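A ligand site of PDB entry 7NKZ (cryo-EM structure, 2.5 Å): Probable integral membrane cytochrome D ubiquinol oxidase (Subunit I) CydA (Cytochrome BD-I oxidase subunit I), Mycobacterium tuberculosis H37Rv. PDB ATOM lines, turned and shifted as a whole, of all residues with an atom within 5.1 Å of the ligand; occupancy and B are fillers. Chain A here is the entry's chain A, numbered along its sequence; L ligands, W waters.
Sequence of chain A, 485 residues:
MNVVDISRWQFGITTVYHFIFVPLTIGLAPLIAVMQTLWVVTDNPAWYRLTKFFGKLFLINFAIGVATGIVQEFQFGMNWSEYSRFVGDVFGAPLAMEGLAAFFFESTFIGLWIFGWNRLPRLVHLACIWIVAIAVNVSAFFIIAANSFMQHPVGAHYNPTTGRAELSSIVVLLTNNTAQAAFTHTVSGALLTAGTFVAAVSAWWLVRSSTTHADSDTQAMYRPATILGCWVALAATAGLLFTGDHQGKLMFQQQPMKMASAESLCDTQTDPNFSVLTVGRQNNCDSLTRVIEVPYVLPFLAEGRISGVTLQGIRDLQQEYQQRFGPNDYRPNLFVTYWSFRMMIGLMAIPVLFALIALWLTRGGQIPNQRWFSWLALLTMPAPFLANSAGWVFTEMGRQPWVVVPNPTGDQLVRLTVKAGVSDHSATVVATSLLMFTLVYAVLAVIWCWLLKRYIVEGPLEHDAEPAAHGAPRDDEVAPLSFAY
The side-chain sulfur (SD) of Met 344 is bound to an iron atom (FE1) of the ligand.
FE1 of the ligand is bound by NE2 of His 185 (2.6 Å).
NE2 of Gln 247 lies within hydrogen-bond range of O4 of the ligand, at 2.7 Å.
O1 of the ligand lies within hydrogen-bond range of OG1 of Thr 395 (3.0 Å).
NZ of Lys 258 is in salt-bridge range of O1 of the ligand (3.3 Å).
A ring nitrogen (ND1) of His 185 is in hydrogen-bond range of the backbone NH (N) of Gly 244 (3.2 Å).
The backbone carbonyl oxygen (O) of Thr 395 lies within hydrogen-bond range of the side-chain amino group (NZ) of Lys 258.
The side-chain hydroxyl of Thr 395 is in hydrogen-bond range of the backbone carbonyl oxygen of Gly 391 (3.0 Å).
The side-chain amide nitrogen of Asn 388 sits at hydrogen-bond distance from the backbone carbonyl oxygen of Gly 189 (3.3 Å).
O of Pro 384 lies within hydrogen-bond range of ND2 of Asn 388 (2.9 Å).
OG1 of Thr 193 sits at hydrogen-bond distance from ND2 of Asn 388, at 2.4 Å.
OG1 of Thr 186 sits at hydrogen-bond distance from O of Ala 182, 2.7 Å away.
The side-chain hydroxyl (OG1) of Thr 193 is in hydrogen-bond range of the backbone carbonyl oxygen (O) of Gly 189, 3.1 Å away.
O of Ala 182 sits close to O3 of the ligand (3.4 Å).
Residues that only touch the ligand: Phe 19, Thr 186, Gly 189, Leu 192, Leu 240, Gly 244, Gly 248, Met 251, Ile 345, Met 348, Ala 387, Asn 388, Gly 391, Trp 392 and Phe 394.
Hydrophobic or aromatic side chains within 4 Å of the ligand: Phe 19, Ala 182, His 185, Leu 192, Leu 240, Met 251, Met 344, Ile 345, Met 348, Ala 387, Trp 392 and Phe 394.
21 residues have an atom within 4 Å of the ligand: Phe 19, Ala 182, His 185, Thr 186, Gly 189, Leu 192, Leu 240, Gly 244, Gln 247, Gly 248, Met 251, Lys 258, Met 344, Ile 345, Met 348, Ala 387, Asn 388, Gly 391, Trp 392, Phe 394 and Thr 395.
Water W1 lies within hydrogen-bond range of an oxygen (O2) of the ligand and the backbone carbonyl oxygen of Gln 247.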
ATOM      1  N   PHE A  19     -30.505  19.702  -6.711  1.00  0.00           N
ATOM      2  CA  PHE A  19     -29.647  19.233  -7.795  1.00  0.00           C
ATOM      3  C   PHE A  19     -28.849  17.994  -7.411  1.00  0.00           C
ATOM      4  O   PHE A  19     -27.863  17.673  -8.089  1.00  0.00           O
ATOM      5  CB  PHE A  19     -28.702  20.352  -8.249  1.00  0.00           C
ATOM      6  CG  PHE A  19     -28.277  20.225  -9.684  1.00  0.00           C
ATOM      7  CD1 PHE A  19     -29.226  20.155 -10.689  1.00  0.00           C
ATOM      8  CD2 PHE A  19     -26.939  20.165 -10.031  1.00  0.00           C
ATOM      9  CE1 PHE A  19     -28.847  20.046 -12.017  1.00  0.00           C
ATOM     10  CE2 PHE A  19     -26.553  20.048 -11.350  1.00  0.00           C
ATOM     11  CZ  PHE A  19     -27.513  19.983 -12.342  1.00  0.00           C
ATOM     12  N   ALA A 181     -25.744  27.113 -24.396  1.00  0.00           N
ATOM     13  CA  ALA A 181     -24.508  26.486 -23.945  1.00  0.00           C
ATOM     14  C   ALA A 181     -24.695  25.791 -22.604  1.00  0.00           C
ATOM     15  O   ALA A 181     -24.178  24.688 -22.396  1.00  0.00           O
ATOM     16  CB  ALA A 181     -23.393  27.526 -23.878  1.00  0.00           C
ATOM     17  N   ALA A 182     -25.413  26.431 -21.685  1.00  0.00           N
ATOM     18  CA  ALA A 182     -25.607  25.832 -20.359  1.00  0.00           C
ATOM     19  C   ALA A 182     -26.605  24.686 -20.395  1.00  0.00           C
ATOM     20  O   ALA A 182     -26.469  23.719 -19.631  1.00  0.00           O
ATOM     21  CB  ALA A 182     -26.065  26.901 -19.362  1.00  0.00           C
ATOM     22  N   HIS A 185     -24.855  21.662 -21.815  1.00  0.00           N
ATOM     23  CA  HIS A 185     -23.830  21.225 -20.878  1.00  0.00           C
ATOM     24  C   HIS A 185     -24.442  20.519 -19.670  1.00  0.00           C
ATOM     25  O   HIS A 185     -23.918  19.504 -19.217  1.00  0.00           O
ATOM     26  CB  HIS A 185     -22.988  22.413 -20.433  1.00  0.00           C
ATOM     27  CG  HIS A 185     -21.709  22.018 -19.758  1.00  0.00           C
ATOM     28  ND1 HIS A 185     -20.675  21.410 -20.432  1.00  0.00           N
ATOM     29  CD2 HIS A 185     -21.306  22.149 -18.472  1.00  0.00           C
ATOM     30  CE1 HIS A 185     -19.680  21.178 -19.595  1.00  0.00           C
ATOM     31  NE2 HIS A 185     -20.036  21.614 -18.394  1.00  0.00           N
ATOM     32  N   THR A 186     -25.542  21.049 -19.140  1.00  0.00           N
ATOM     33  CA  THR A 186     -26.207  20.415 -18.013  1.00  0.00           C
ATOM     34  C   THR A 186     -26.812  19.072 -18.408  1.00  0.00           C
ATOM     35  O   THR A 186     -26.748  18.109 -17.639  1.00  0.00           O
ATOM     36  CB  THR A 186     -27.279  21.342 -17.430  1.00  0.00           C
ATOM     37  OG1 THR A 186     -26.698  22.625 -17.156  1.00  0.00           O
ATOM     38  CG2 THR A 186     -27.844  20.772 -16.143  1.00  0.00           C
ATOM     39  N   GLY A 189     -24.085  16.836 -18.598  1.00  0.00           N
ATOM     40  CA  GLY A 189     -23.739  16.500 -17.224  1.00  0.00           C
ATOM     41  C   GLY A 189     -24.714  15.536 -16.582  1.00  0.00           C
ATOM     42  O   GLY A 189     -24.309  14.665 -15.805  1.00  0.00           O
ATOM     43  N   ALA A 190     -26.000  15.683 -16.890  1.00  0.00           N
ATOM     44  CA  ALA A 190     -26.998  14.765 -16.349  1.00  0.00           C
ATOM     45  C   ALA A 190     -26.847  13.356 -16.923  1.00  0.00           C
ATOM     46  O   ALA A 190     -27.059  12.373 -16.208  1.00  0.00           O
ATOM     47  CB  ALA A 190     -28.402  15.297 -16.619  1.00  0.00           C
ATOM     48  N   LEU A 192     -24.026  11.959 -17.813  1.00  0.00           N
ATOM     49  CA  LEU A 192     -22.902  11.357 -17.111  1.00  0.00           C
ATOM     50  C   LEU A 192     -23.314  10.845 -15.738  1.00  0.00           C
ATOM     51  O   LEU A 192     -22.861   9.769 -15.310  1.00  0.00           O
ATOM     52  CB  LEU A 192     -21.757  12.357 -16.973  1.00  0.00           C
ATOM     53  CG  LEU A 192     -20.510  11.860 -16.250  1.00  0.00           C
ATOM     54  CD1 LEU A 192     -19.820  10.768 -17.051  1.00  0.00           C
ATOM     55  CD2 LEU A 192     -19.547  13.004 -15.955  1.00  0.00           C
ATOM     56  N   THR A 193     -24.168  11.591 -15.027  1.00  0.00           N
ATOM     57  CA  THR A 193     -24.604  11.165 -13.705  1.00  0.00           C
ATOM     58  C   THR A 193     -25.392   9.863 -13.774  1.00  0.00           C
ATOM     59  O   THR A 193     -25.148   8.931 -12.990  1.00  0.00           O
ATOM     60  CB  THR A 193     -25.443  12.261 -13.048  1.00  0.00           C
ATOM     61  OG1 THR A 193     -24.662  13.459 -12.949  1.00  0.00           O
ATOM     62  CG2 THR A 193     -25.888  11.841 -11.662  1.00  0.00           C
ATOM     63  N   LEU A 240     -19.527  16.939 -22.558  1.00  0.00           N
ATOM     64  CA  LEU A 240     -19.120  17.902 -21.536  1.00  0.00           C
ATOM     65  C   LEU A 240     -17.881  18.682 -21.965  1.00  0.00           C
ATOM     66  O   LEU A 240     -17.744  19.857 -21.608  1.00  0.00           O
ATOM     67  CB  LEU A 240     -18.870  17.188 -20.215  1.00  0.00           C
ATOM     68  CG  LEU A 240     -20.113  16.771 -19.429  1.00  0.00           C
ATOM     69  CD1 LEU A 240     -19.758  15.788 -18.334  1.00  0.00           C
ATOM     70  CD2 LEU A 240     -20.805  17.993 -18.854  1.00  0.00           C
ATOM     71  N   LEU A 241     -16.964  18.048 -22.706  1.00  0.00           N
ATOM     72  CA  LEU A 241     -15.801  18.761 -23.203  1.00  0.00           C
ATOM     73  C   LEU A 241     -16.183  19.779 -24.272  1.00  0.00           C
ATOM     74  O   LEU A 241     -15.692  20.917 -24.256  1.00  0.00           O
ATOM     75  CB  LEU A 241     -14.779  17.771 -23.757  1.00  0.00           C
ATOM     76  CG  LEU A 241     -14.080  16.868 -22.745  1.00  0.00           C
ATOM     77  CD1 LEU A 241     -13.155  15.890 -23.446  1.00  0.00           C
ATOM     78  CD2 LEU A 241     -13.313  17.706 -21.736  1.00  0.00           C
ATOM     79  N   GLY A 244     -18.461  22.288 -22.529  1.00  0.00           N
ATOM     80  CA  GLY A 244     -17.587  23.013 -21.621  1.00  0.00           C
ATOM     81  C   GLY A 244     -16.669  23.985 -22.337  1.00  0.00           C
ATOM     82  O   GLY A 244     -16.316  25.030 -21.785  1.00  0.00           O
ATOM     83  N   GLN A 247     -18.965  26.980 -23.207  1.00  0.00           N
ATOM     84  CA  GLN A 247     -19.238  27.812 -22.033  1.00  0.00           C
ATOM     85  C   GLN A 247     -18.120  28.714 -21.511  1.00  0.00           C
ATOM     86  O   GLN A 247     -18.371  29.837 -21.091  1.00  0.00           O
ATOM     87  CB  GLN A 247     -19.779  26.958 -20.885  1.00  0.00           C
ATOM     88  CG  GLN A 247     -21.289  26.885 -20.852  1.00  0.00           C
ATOM     89  CD  GLN A 247     -21.801  26.333 -19.548  1.00  0.00           C
ATOM     90  OE1 GLN A 247     -21.377  25.284 -19.101  1.00  0.00           O
ATOM     91  NE2 GLN A 247     -22.726  27.057 -18.936  1.00  0.00           N
ATOM     92  N   GLY A 248     -16.871  28.231 -21.542  1.00  0.00           N
ATOM     93  CA  GLY A 248     -15.755  29.034 -21.072  1.00  0.00           C
ATOM     94  C   GLY A 248     -15.568  30.286 -21.894  1.00  0.00           C
ATOM     95  O   GLY A 248     -15.299  31.381 -21.386  1.00  0.00           O
ATOM     96  N   MET A 251     -18.142  32.736 -20.950  1.00  0.00           N
ATOM     97  CA  MET A 251     -17.761  33.280 -19.663  1.00  0.00           C
ATOM     98  C   MET A 251     -16.737  34.391 -19.813  1.00  0.00           C
ATOM     99  O   MET A 251     -16.787  35.383 -19.104  1.00  0.00           O
ATOM    100  CB  MET A 251     -17.214  32.154 -18.782  1.00  0.00           C
ATOM    101  CG  MET A 251     -16.725  32.588 -17.421  1.00  0.00           C
ATOM    102  SD  MET A 251     -16.401  31.160 -16.363  1.00  0.00           S
ATOM    103  CE  MET A 251     -15.086  30.337 -17.245  1.00  0.00           C
ATOM    104  N   LYS A 258     -15.957  36.226 -13.315  1.00  0.00           N
ATOM    105  CA  LYS A 258     -16.079  34.784 -13.100  1.00  0.00           C
ATOM    106  C   LYS A 258     -14.971  34.010 -13.808  1.00  0.00           C
ATOM    107  O   LYS A 258     -14.512  32.986 -13.296  1.00  0.00           O
ATOM    108  CB  LYS A 258     -17.455  34.300 -13.572  1.00  0.00           C
ATOM    109  CG  LYS A 258     -17.763  32.865 -13.178  1.00  0.00           C
ATOM    110  CD  LYS A 258     -19.116  32.428 -13.723  1.00  0.00           C
ATOM    111  CE  LYS A 258     -20.257  33.167 -13.048  1.00  0.00           C
ATOM    112  NZ  LYS A 258     -21.579  32.740 -13.577  1.00  0.00           N
ATOM    113  N   LEU A 301      -9.461  27.760 -23.029  1.00  0.00           N
ATOM    114  CA  LEU A 301     -10.828  27.890 -22.548  1.00  0.00           C
ATOM    115  C   LEU A 301     -11.381  29.304 -22.691  1.00  0.00           C
ATOM    116  O   LEU A 301     -12.600  29.461 -22.774  1.00  0.00           O
ATOM    117  CB  LEU A 301     -10.908  27.443 -21.088  1.00  0.00           C
ATOM    118  CG  LEU A 301     -12.300  27.304 -20.456  1.00  0.00           C
ATOM    119  CD1 LEU A 301     -13.115  26.250 -21.175  1.00  0.00           C
ATOM    120  CD2 LEU A 301     -12.198  26.992 -18.972  1.00  0.00           C
ATOM    121  N   PHE A 341     -14.247  24.880  -8.559  1.00  0.00           N
ATOM    122  CA  PHE A 341     -13.881  24.701  -9.961  1.00  0.00           C
ATOM    123  C   PHE A 341     -12.851  23.587 -10.137  1.00  0.00           C
ATOM    124  O   PHE A 341     -12.854  22.898 -11.160  1.00  0.00           O
ATOM    125  CB  PHE A 341     -13.339  26.021 -10.526  1.00  0.00           C
ATOM    126  CG  PHE A 341     -13.189  26.013 -12.023  1.00  0.00           C
ATOM    127  CD1 PHE A 341     -14.280  26.252 -12.837  1.00  0.00           C
ATOM    128  CD2 PHE A 341     -11.960  25.779 -12.616  1.00  0.00           C
ATOM    129  CE1 PHE A 341     -14.149  26.250 -14.214  1.00  0.00           C
ATOM    130  CE2 PHE A 341     -11.819  25.782 -13.985  1.00  0.00           C
ATOM    131  CZ  PHE A 341     -12.922  26.018 -14.792  1.00  0.00           C
ATOM    132  N   MET A 344     -15.254  20.520 -10.076  1.00  0.00           N
ATOM    133  CA  MET A 344     -16.062  20.171 -11.227  1.00  0.00           C
ATOM    134  C   MET A 344     -15.219  19.440 -12.264  1.00  0.00           C
ATOM    135  O   MET A 344     -15.616  18.414 -12.782  1.00  0.00           O
ATOM    136  CB  MET A 344     -16.621  21.451 -11.852  1.00  0.00           C
ATOM    137  CG  MET A 344     -17.727  21.234 -12.867  1.00  0.00           C
ATOM    138  SD  MET A 344     -17.756  22.509 -14.137  1.00  0.00           S
ATOM    139  CE  MET A 344     -16.647  23.723 -13.467  1.00  0.00           C
ATOM    140  N   ILE A 345     -14.045  19.998 -12.549  1.00  0.00           N
ATOM    141  CA  ILE A 345     -13.100  19.411 -13.509  1.00  0.00           C
ATOM    142  C   ILE A 345     -12.401  18.111 -13.110  1.00  0.00           C
ATOM    143  O   ILE A 345     -12.324  17.180 -13.894  1.00  0.00           O
ATOM    144  CB  ILE A 345     -12.005  20.433 -13.878  1.00  0.00           C
ATOM    145  CG1 ILE A 345     -12.603  21.800 -14.177  1.00  0.00           C
ATOM    146  CG2 ILE A 345     -11.191  19.921 -15.054  1.00  0.00           C
ATOM    147  CD1 ILE A 345     -13.293  21.884 -15.504  1.00  0.00           C
ATOM    148  N   LEU A 347     -13.192  15.814 -10.975  1.00  0.00           N
ATOM    149  CA  LEU A 347     -14.155  14.738 -10.832  1.00  0.00           C
ATOM    150  C   LEU A 347     -14.575  14.121 -12.166  1.00  0.00           C
ATOM    151  O   LEU A 347     -15.576  13.393 -12.193  1.00  0.00           O
ATOM    152  CB  LEU A 347     -15.393  15.242 -10.081  1.00  0.00           C
ATOM    153  CG  LEU A 347     -15.236  15.346  -8.559  1.00  0.00           C
ATOM    154  CD1 LEU A 347     -16.506  15.896  -7.924  1.00  0.00           C
ATOM    155  CD2 LEU A 347     -14.863  14.005  -7.959  1.00  0.00           C
ATOM    156  N   MET A 348     -13.863  14.394 -13.251  1.00  0.00           N
ATOM    157  CA  MET A 348     -14.068  13.651 -14.486  1.00  0.00           C
ATOM    158  C   MET A 348     -13.294  12.339 -14.527  1.00  0.00           C
ATOM    159  O   MET A 348     -13.732  11.394 -15.177  1.00  0.00           O
ATOM    160  CB  MET A 348     -13.674  14.486 -15.707  1.00  0.00           C
ATOM    161  CG  MET A 348     -14.633  15.595 -16.054  1.00  0.00           C
ATOM    162  SD  MET A 348     -15.571  15.194 -17.538  1.00  0.00           S
ATOM    163  CE  MET A 348     -14.562  15.950 -18.809  1.00  0.00           C
ATOM    164  N   PRO A 384     -20.097  11.900 -10.176  1.00  0.00           N
ATOM    165  CA  PRO A 384     -20.873  12.842 -11.003  1.00  0.00           C
ATOM    166  C   PRO A 384     -21.885  13.645 -10.209  1.00  0.00           C
ATOM    167  O   PRO A 384     -22.185  14.793 -10.589  1.00  0.00           O
ATOM    168  CB  PRO A 384     -21.558  11.935 -12.029  1.00  0.00           C
ATOM    169  CG  PRO A 384     -20.818  10.643 -11.970  1.00  0.00           C
ATOM    170  CD  PRO A 384     -20.384  10.509 -10.548  1.00  0.00           C
ATOM    171  N   ALA A 387     -19.793  16.397  -8.809  1.00  0.00           N
ATOM    172  CA  ALA A 387     -19.304  17.257  -9.885  1.00  0.00           C
ATOM    173  C   ALA A 387     -20.411  18.171 -10.405  1.00  0.00           C
ATOM    174  O   ALA A 387     -20.156  19.347 -10.712  1.00  0.00           O
ATOM    175  CB  ALA A 387     -18.733  16.400 -11.016  1.00  0.00           C
ATOM    176  N   ASN A 388     -21.630  17.644 -10.534  1.00  0.00           N
ATOM    177  CA  ASN A 388     -22.750  18.483 -10.958  1.00  0.00           C
ATOM    178  C   ASN A 388     -23.050  19.574  -9.946  1.00  0.00           C
ATOM    179  O   ASN A 388     -23.363  20.703 -10.331  1.00  0.00           O
ATOM    180  CB  ASN A 388     -23.985  17.606 -11.194  1.00  0.00           C
ATOM    181  CG  ASN A 388     -24.047  17.047 -12.597  1.00  0.00           C
ATOM    182  OD1 ASN A 388     -24.218  17.793 -13.564  1.00  0.00           O
ATOM    183  ND2 ASN A 388     -23.916  15.730 -12.712  1.00  0.00           N
ATOM    184  N   GLY A 391     -20.376  22.261 -10.312  1.00  0.00           N
ATOM    185  CA  GLY A 391     -20.492  23.058 -11.524  1.00  0.00           C
ATOM    186  C   GLY A 391     -21.454  24.214 -11.386  1.00  0.00           C
ATOM    187  O   GLY A 391     -21.160  25.337 -11.800  1.00  0.00           O
ATOM    188  N   TRP A 392     -22.633  23.958 -10.810  1.00  0.00           N
ATOM    189  CA  TRP A 392     -23.611  25.029 -10.632  1.00  0.00           C
ATOM    190  C   TRP A 392     -23.214  25.976  -9.513  1.00  0.00           C
ATOM    191  O   TRP A 392     -23.568  27.159  -9.543  1.00  0.00           O
ATOM    192  CB  TRP A 392     -24.988  24.432 -10.364  1.00  0.00           C
ATOM    193  CG  TRP A 392     -25.921  24.445 -11.531  1.00  0.00           C
ATOM    194  CD1 TRP A 392     -26.331  23.374 -12.267  1.00  0.00           C
ATOM    195  CD2 TRP A 392     -26.574  25.592 -12.088  1.00  0.00           C
ATOM    196  NE1 TRP A 392     -27.196  23.790 -13.252  1.00  0.00           N
ATOM    197  CE2 TRP A 392     -27.358  25.139 -13.162  1.00  0.00           C
ATOM    198  CE3 TRP A 392     -26.562  26.960 -11.783  1.00  0.00           C
ATOM    199  CZ2 TRP A 392     -28.129  26.000 -13.941  1.00  0.00           C
ATOM    200  CZ3 TRP A 392     -27.324  27.819 -12.560  1.00  0.00           C
ATOM    201  CH2 TRP A 392     -28.095  27.335 -13.625  1.00  0.00           C
ATOM    202  N   PHE A 394     -20.136  27.001  -8.809  1.00  0.00           N
ATOM    203  CA  PHE A 394     -19.237  27.967  -9.425  1.00  0.00           C
ATOM    204  C   PHE A 394     -19.995  28.985 -10.259  1.00  0.00           C
ATOM    205  O   PHE A 394     -19.595  30.151 -10.340  1.00  0.00           O
ATOM    206  CB  PHE A 394     -18.195  27.250 -10.278  1.00  0.00           C
ATOM    207  CG  PHE A 394     -17.361  28.169 -11.118  1.00  0.00           C
ATOM    208  CD1 PHE A 394     -16.330  28.899 -10.562  1.00  0.00           C
ATOM    209  CD2 PHE A 394     -17.618  28.306 -12.481  1.00  0.00           C
ATOM    210  CE1 PHE A 394     -15.562  29.757 -11.339  1.00  0.00           C
ATOM    211  CE2 PHE A 394     -16.854  29.151 -13.255  1.00  0.00           C
ATOM    212  CZ  PHE A 394     -15.835  29.878 -12.693  1.00  0.00           C
ATOM    213  N   THR A 395     -21.100  28.566 -10.885  1.00  0.00           N
ATOM    214  CA  THR A 395     -21.907  29.494 -11.669  1.00  0.00           C
ATOM    215  C   THR A 395     -22.571  30.537 -10.781  1.00  0.00           C
ATOM    216  O   THR A 395     -22.648  31.713 -11.145  1.00  0.00           O
ATOM    217  CB  THR A 395     -22.955  28.721 -12.480  1.00  0.00           C
ATOM    218  OG1 THR A 395     -22.301  27.716 -13.261  1.00  0.00           O
ATOM    219  CG2 THR A 395     -23.713  29.664 -13.399  1.00  0.00           C
HETATM  220 FE1  LIG L   1     -18.679  22.038 -16.254  1.00  0.00          FE
HETATM  221  C1  LIG L   1     -20.737  25.143 -15.929  1.00  0.00           C
HETATM  222  C2  LIG L   1     -16.091  23.894 -18.119  1.00  0.00           C
HETATM  223  C3  LIG L   1     -16.704  18.924 -16.538  1.00  0.00           C
HETATM  224  C4  LIG L   1     -21.289  20.032 -14.345  1.00  0.00           C
HETATM  225  N1  LIG L   1     -18.511  24.069 -16.864  1.00  0.00           N
HETATM  226  C5  LIG L   1     -19.446  25.147 -16.631  1.00  0.00           C
HETATM  227  C6  LIG L   1     -18.787  26.127 -17.230  1.00  0.00           C
HETATM  228  C7  LIG L   1     -17.686  25.920 -17.772  1.00  0.00           C
HETATM  229  C8  LIG L   1     -17.299  24.625 -17.655  1.00  0.00           C
HETATM  230  C9  LIG L   1     -16.869  27.000 -18.489  1.00  0.00           C
HETATM  231  C10 LIG L   1     -19.393  27.531 -17.261  1.00  0.00           C
HETATM  232  C11 LIG L   1     -19.239  28.227 -15.913  1.00  0.00           C
HETATM  233  C12 LIG L   1     -20.277  29.335 -15.817  1.00  0.00           C
HETATM  234  O1  LIG L   1     -20.633  29.758 -14.687  1.00  0.00           O
HETATM  235  O2  LIG L   1     -20.782  29.826 -16.860  1.00  0.00           O
HETATM  236  N2  LIG L   1     -16.785  21.516 -17.150  1.00  0.00           N
HETATM  237  C13 LIG L   1     -15.888  22.442 -17.867  1.00  0.00           C
HETATM  238  C14 LIG L   1     -14.938  21.614 -18.167  1.00  0.00           C
HETATM  239  C15 LIG L   1     -14.994  20.423 -17.831  1.00  0.00           C
HETATM  240  C16 LIG L   1     -16.157  20.147 -17.139  1.00  0.00           C
HETATM  241  C17 LIG L   1     -13.742  22.111 -18.940  1.00  0.00           C
HETATM  242  C18 LIG L   1     -13.927  19.396 -18.160  1.00  0.00           C
HETATM  243  C19 LIG L   1     -13.256  18.888 -16.903  1.00  0.00           C
HETATM  244  N3  LIG L   1     -19.027  20.008 -15.566  1.00  0.00           N
HETATM  245  C20 LIG L   1     -18.039  18.884 -15.811  1.00  0.00           C
HETATM  246  C21 LIG L   1     -18.597  17.934 -15.272  1.00  0.00           C
HETATM  247  C22 LIG L   1     -19.684  18.072 -14.720  1.00  0.00           C
HETATM  248  C23 LIG L   1     -20.145  19.428 -14.809  1.00  0.00           C
HETATM  249  C24 LIG L   1     -17.935  16.569 -15.272  1.00  0.00           C
HETATM  250  C25 LIG L   1     -20.440  16.973 -14.020  1.00  0.00           C
HETATM  251  C26 LIG L   1     -21.334  16.148 -14.938  1.00  0.00           C
HETATM  252  N4  LIG L   1     -20.764  22.452 -15.243  1.00  0.00           N
HETATM  253  C27 LIG L   1     -21.580  21.491 -14.559  1.00  0.00           C
HETATM  254  C28 LIG L   1     -22.572  22.299 -14.223  1.00  0.00           C
HETATM  255  C29 LIG L   1     -22.598  23.640 -14.552  1.00  0.00           C
HETATM  256  C30 LIG L   1     -21.355  23.873 -15.283  1.00  0.00           C
HETATM  257  C31 LIG L   1     -23.724  21.707 -13.461  1.00  0.00           C
HETATM  258  C32 LIG L   1     -23.694  24.672 -14.228  1.00  0.00           C
HETATM  259  C33 LIG L   1     -24.680  24.740 -15.378  1.00  0.00           C
HETATM  260  C34 LIG L   1     -24.037  25.476 -16.545  1.00  0.00           C
HETATM  261  O3  LIG L   1     -23.906  24.901 -17.649  1.00  0.00           O
HETATM  262  O4  LIG L   1     -23.649  26.672 -16.401  1.00  0.00           O
HETATM  263  O   HOH W   1     -20.954  30.813 -19.669  1.00  0.00           O
